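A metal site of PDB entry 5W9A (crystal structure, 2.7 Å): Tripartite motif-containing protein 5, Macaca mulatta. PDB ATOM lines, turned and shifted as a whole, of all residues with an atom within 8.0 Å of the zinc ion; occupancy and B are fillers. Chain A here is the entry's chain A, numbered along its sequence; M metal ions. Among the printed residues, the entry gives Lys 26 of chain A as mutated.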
ATOM      1  N   PHE A  13      -1.525  12.901  -1.256  1.00  0.00           N
ATOM      2  CA  PHE A  13      -2.752  13.454  -1.827  1.00  0.00           C
ATOM      3  C   PHE A  13      -3.489  12.331  -2.519  1.00  0.00           C
ATOM      4  O   PHE A  13      -2.914  11.629  -3.365  1.00  0.00           O
ATOM      5  CB  PHE A  13      -2.434  14.588  -2.806  1.00  0.00           C
ATOM      6  CG  PHE A  13      -3.648  15.239  -3.402  1.00  0.00           C
ATOM      7  CD1 PHE A  13      -4.201  14.765  -4.581  1.00  0.00           C
ATOM      8  CD2 PHE A  13      -4.226  16.346  -2.793  1.00  0.00           C
ATOM      9  CE1 PHE A  13      -5.320  15.375  -5.132  1.00  0.00           C
ATOM     10  CE2 PHE A  13      -5.335  16.947  -3.342  1.00  0.00           C
ATOM     11  CZ  PHE A  13      -5.887  16.467  -4.508  1.00  0.00           C
ATOM     12  N   CYS A  14      -4.758  12.151  -2.174  1.00  0.00           N
ATOM     13  CA  CYS A  14      -5.576  11.101  -2.762  1.00  0.00           C
ATOM     14  C   CYS A  14      -6.358  11.672  -3.944  1.00  0.00           C
ATOM     15  O   CYS A  14      -7.136  12.623  -3.774  1.00  0.00           O
ATOM     16  CB  CYS A  14      -6.532  10.505  -1.726  1.00  0.00           C
ATOM     17  SG  CYS A  14      -7.405   9.028  -2.279  1.00  0.00           S
ATOM     18  N   GLN A  15      -6.135  11.113  -5.130  1.00  0.00           N
ATOM     19  CA  GLN A  15      -6.803  11.615  -6.321  1.00  0.00           C
ATOM     20  C   GLN A  15      -8.313  11.416  -6.251  1.00  0.00           C
ATOM     21  O   GLN A  15      -9.072  12.208  -6.810  1.00  0.00           O
ATOM     22  CB  GLN A  15      -6.235  10.940  -7.570  1.00  0.00           C
ATOM     23  CG  GLN A  15      -6.723  11.527  -8.890  1.00  0.00           C
ATOM     24  CD  GLN A  15      -6.092  10.844 -10.084  1.00  0.00           C
ATOM     25  OE1 GLN A  15      -5.361   9.867  -9.957  1.00  0.00           O
ATOM     26  NE2 GLN A  15      -6.381  11.370 -11.281  1.00  0.00           N
ATOM     27  N   GLU A  16      -8.767  10.366  -5.553  1.00  0.00           N
ATOM     28  CA  GLU A  16     -10.180  10.059  -5.478  1.00  0.00           C
ATOM     29  C   GLU A  16     -10.889  10.824  -4.365  1.00  0.00           C
ATOM     30  O   GLU A  16     -11.971  11.384  -4.581  1.00  0.00           O
ATOM     31  CB  GLU A  16     -10.379   8.549  -5.292  1.00  0.00           C
ATOM     32  N   ASP A  17     -10.291  10.870  -3.174  1.00  0.00           N
ATOM     33  CA  ASP A  17     -10.912  11.523  -2.033  1.00  0.00           C
ATOM     34  C   ASP A  17     -10.579  13.001  -1.914  1.00  0.00           C
ATOM     35  O   ASP A  17     -11.271  13.717  -1.187  1.00  0.00           O
ATOM     36  CB  ASP A  17     -10.518  10.805  -0.739  1.00  0.00           C
ATOM     37  CG  ASP A  17     -11.058   9.391  -0.664  1.00  0.00           C
ATOM     38  OD1 ASP A  17     -12.149   9.144  -1.211  1.00  0.00           O
ATOM     39  OD2 ASP A  17     -10.393   8.526  -0.056  1.00  0.00           O
ATOM     40  N   SER A  18      -9.520  13.462  -2.598  1.00  0.00           N
ATOM     41  CA  SER A  18      -9.074  14.857  -2.526  1.00  0.00           C
ATOM     42  C   SER A  18      -8.738  15.287  -1.094  1.00  0.00           C
ATOM     43  O   SER A  18      -8.929  16.451  -0.736  1.00  0.00           O
ATOM     44  CB  SER A  18     -10.105  15.810  -3.147  1.00  0.00           C
ATOM     45  OG  SER A  18      -9.759  17.163  -2.899  1.00  0.00           O
ATOM     46  N   LYS A  19      -8.252  14.364  -0.281  1.00  0.00           N
ATOM     47  CA  LYS A  19      -7.842  14.658   1.081  1.00  0.00           C
ATOM     48  C   LYS A  19      -6.371  14.307   1.269  1.00  0.00           C
ATOM     49  O   LYS A  19      -5.903  13.274   0.774  1.00  0.00           O
ATOM     50  CB  LYS A  19      -8.689  13.884   2.103  1.00  0.00           C
ATOM     51  CG  LYS A  19     -10.171  14.193   2.069  1.00  0.00           C
ATOM     52  CD  LYS A  19     -10.899  13.526   3.221  1.00  0.00           C
ATOM     53  CE  LYS A  19     -10.685  12.021   3.216  1.00  0.00           C
ATOM     54  NZ  LYS A  19     -11.352  11.361   4.375  1.00  0.00           N
ATOM     55  N   VAL A  20      -5.648  15.160   1.982  1.00  0.00           N
ATOM     56  CA  VAL A  20      -4.254  14.866   2.320  1.00  0.00           C
ATOM     57  C   VAL A  20      -4.223  13.942   3.525  1.00  0.00           C
ATOM     58  O   VAL A  20      -4.976  14.124   4.495  1.00  0.00           O
ATOM     59  CB  VAL A  20      -3.465  16.169   2.576  1.00  0.00           C
ATOM     60  CG1 VAL A  20      -3.341  16.971   1.294  1.00  0.00           C
ATOM     61  CG2 VAL A  20      -4.117  16.995   3.667  1.00  0.00           C
ATOM     62  N   ILE A  21      -3.367  12.919   3.464  1.00  0.00           N
ATOM     63  CA  ILE A  21      -3.307  11.899   4.511  1.00  0.00           C
ATOM     64  C   ILE A  21      -1.853  11.523   4.751  1.00  0.00           C
ATOM     65  O   ILE A  21      -0.938  12.155   4.222  1.00  0.00           O
ATOM     66  CB  ILE A  21      -4.136  10.665   4.126  1.00  0.00           C
ATOM     67  CG1 ILE A  21      -3.777  10.195   2.714  1.00  0.00           C
ATOM     68  CG2 ILE A  21      -5.630  10.944   4.251  1.00  0.00           C
ATOM     69  CD1 ILE A  21      -4.507   8.950   2.278  1.00  0.00           C
ATOM     70  N   CYS A  25      -2.700   5.940   6.566  1.00  0.00           N
ATOM     71  CA  CYS A  25      -4.050   6.039   6.029  1.00  0.00           C
ATOM     72  C   CYS A  25      -4.181   5.396   4.647  1.00  0.00           C
ATOM     73  O   CYS A  25      -5.291   5.039   4.245  1.00  0.00           O
ATOM     74  CB  CYS A  25      -4.487   7.508   5.945  1.00  0.00           C
ATOM     75  SG  CYS A  25      -4.520   8.373   7.540  1.00  0.00           S
ATOM     76  N   LYS A  26      -3.071   5.261   3.918  1.00  0.00           N
ATOM     77  CA  LYS A  26      -3.144   4.679   2.576  1.00  0.00           C
ATOM     78  C   LYS A  26      -3.389   3.177   2.612  1.00  0.00           C
ATOM     79  O   LYS A  26      -4.067   2.641   1.733  1.00  0.00           O
ATOM     80  CB  LYS A  26      -1.849   4.991   1.813  1.00  0.00           C
ATOM     81  CG  LYS A  26      -1.886   4.571   0.350  1.00  0.00           C
ATOM     82  CD  LYS A  26      -0.603   4.949  -0.373  1.00  0.00           C
ATOM     83  CE  LYS A  26       0.594   4.199   0.184  1.00  0.00           C
ATOM     84  NZ  LYS A  26       1.840   4.505  -0.555  1.00  0.00           N
ATOM     85  N   SER A  28      -4.882   1.488   5.211  1.00  0.00           N
ATOM     86  CA  SER A  28      -6.096   1.129   5.915  1.00  0.00           C
ATOM     87  C   SER A  28      -7.274   1.035   4.944  1.00  0.00           C
ATOM     88  O   SER A  28      -7.183   1.419   3.779  1.00  0.00           O
ATOM     89  CB  SER A  28      -6.388   2.146   7.026  1.00  0.00           C
ATOM     90  OG  SER A  28      -6.672   3.421   6.477  1.00  0.00           O
ATOM     91  N   GLN A  29      -8.397   0.530   5.454  1.00  0.00           N
ATOM     92  CA  GLN A  29      -9.585   0.368   4.624  1.00  0.00           C
ATOM     93  C   GLN A  29     -10.226   1.692   4.257  1.00  0.00           C
ATOM     94  O   GLN A  29     -11.038   1.733   3.326  1.00  0.00           O
ATOM     95  CB  GLN A  29     -10.609  -0.525   5.342  1.00  0.00           C
ATOM     96  N   GLU A  30      -9.887   2.779   4.959  1.00  0.00           N
ATOM     97  CA  GLU A  30     -10.502   4.071   4.676  1.00  0.00           C
ATOM     98  C   GLU A  30     -10.106   4.588   3.287  1.00  0.00           C
ATOM     99  O   GLU A  30     -10.957   5.099   2.552  1.00  0.00           O
ATOM    100  CB  GLU A  30     -10.113   5.085   5.763  1.00  0.00           C
ATOM    101  CG  GLU A  30     -10.161   6.549   5.344  1.00  0.00           C
ATOM    102  CD  GLU A  30     -11.561   7.120   5.226  1.00  0.00           C
ATOM    103  OE1 GLU A  30     -12.491   6.400   4.810  1.00  0.00           O
ATOM    104  OE2 GLU A  30     -11.725   8.317   5.550  1.00  0.00           O
ATOM    105  N   HIS A  31      -8.831   4.452   2.915  1.00  0.00           N
ATOM    106  CA  HIS A  31      -8.357   4.887   1.607  1.00  0.00           C
ATOM    107  C   HIS A  31      -7.774   3.723   0.806  1.00  0.00           C
ATOM    108  O   HIS A  31      -6.854   3.902   0.013  1.00  0.00           O
ATOM    109  CB  HIS A  31      -7.323   6.008   1.720  1.00  0.00           C
ATOM    110  CG  HIS A  31      -7.776   7.182   2.525  1.00  0.00           C
ATOM    111  ND1 HIS A  31      -8.623   8.144   2.014  1.00  0.00           N
ATOM    112  CD2 HIS A  31      -7.467   7.589   3.775  1.00  0.00           C
ATOM    113  CE1 HIS A  31      -8.838   9.077   2.930  1.00  0.00           C
ATOM    114  NE2 HIS A  31      -8.145   8.758   4.003  1.00  0.00           N
ATOM    115  N   ARG A  32      -8.299   2.518   1.019  1.00  0.00           N
ATOM    116  CA  ARG A  32      -7.791   1.349   0.338  1.00  0.00           C
ATOM    117  C   ARG A  32      -8.183   1.355  -1.140  1.00  0.00           C
ATOM    118  O   ARG A  32      -9.293   1.756  -1.502  1.00  0.00           O
ATOM    119  CB  ARG A  32      -8.304   0.069   1.001  1.00  0.00           C
ATOM    120  N   GLY A  33      -7.251   0.919  -1.993  1.00  0.00           N
ATOM    121  CA  GLY A  33      -7.503   0.786  -3.414  1.00  0.00           C
ATOM    122  C   GLY A  33      -7.436   2.057  -4.224  1.00  0.00           C
ATOM    123  O   GLY A  33      -7.533   1.992  -5.450  1.00  0.00           O
ATOM    124  N   HIS A  34      -7.274   3.216  -3.586  1.00  0.00           N
ATOM    125  CA  HIS A  34      -7.234   4.471  -4.315  1.00  0.00           C
ATOM    126  C   HIS A  34      -5.828   4.742  -4.854  1.00  0.00           C
ATOM    127  O   HIS A  34      -4.864   4.063  -4.530  1.00  0.00           O
ATOM    128  CB  HIS A  34      -7.694   5.631  -3.431  1.00  0.00           C
ATOM    129  CG  HIS A  34      -9.052   5.446  -2.838  1.00  0.00           C
ATOM    130  ND1 HIS A  34      -9.560   6.280  -1.870  1.00  0.00           N
ATOM    131  CD2 HIS A  34     -10.014   4.526  -3.088  1.00  0.00           C
ATOM    132  CE1 HIS A  34     -10.778   5.884  -1.545  1.00  0.00           C
ATOM    133  NE2 HIS A  34     -11.078   4.817  -2.255  1.00  0.00           N
ATOM    134  N   HIS A  35      -5.739   5.754  -5.711  1.00  0.00           N
ATOM    135  CA  HIS A  35      -4.464   6.198  -6.276  1.00  0.00           C
ATOM    136  C   HIS A  35      -3.956   7.388  -5.466  1.00  0.00           C
ATOM    137  O   HIS A  35      -4.675   8.377  -5.290  1.00  0.00           O
ATOM    138  CB  HIS A  35      -4.615   6.576  -7.742  1.00  0.00           C
ATOM    139  N   THR A  36      -2.717   7.282  -4.988  1.00  0.00           N
ATOM    140  CA  THR A  36      -2.135   8.281  -4.101  1.00  0.00           C
ATOM    141  C   THR A  36      -0.869   8.857  -4.713  1.00  0.00           C
ATOM    142  O   THR A  36      -0.049   8.116  -5.265  1.00  0.00           O
ATOM    143  CB  THR A  36      -1.824   7.670  -2.726  1.00  0.00           C
ATOM    144  OG1 THR A  36      -2.946   6.914  -2.266  1.00  0.00           O
ATOM    145  CG2 THR A  36      -1.503   8.759  -1.717  1.00  0.00           C
HETATM  146 ZN    ZN M   1      -8.456   8.138  -0.278  1.00  0.00          ZN
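The side-chain carboxylate of Asp 17 lies close to a ring nitrogen (ND1) of His 34, 3.0 Å away.
The side-chain sulfur of Cys 14 sits close to a ring nitrogen (ND1) of His 34 (3.5 Å).
SG of Cys 14 sits close to N of Glu 16, at 3.8 Å.
The backbone carbonyl oxygen (O) of Lys 19 is in hydrogen-bond range of the backbone NH (N) of Cys 14 (3.4 Å).
Of the 20 residues printed, 4 come within 4 Å of the zinc ion.
The nearest printed residue that does not touch the zinc ion is Ile 21 (4.8 Å).
The zinc ion is bound by the side-chain carboxylate (OD2) of Asp 17 (2.0 Å).
A ring nitrogen (ND1) of His 31 is bound to the zinc ion (2.3 Å).
The zinc ion is bound by SG of Cys 14, 2.4 Å away.
Slightly farther from the zinc ion lies ND1 of His 34 (2.7 Å).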
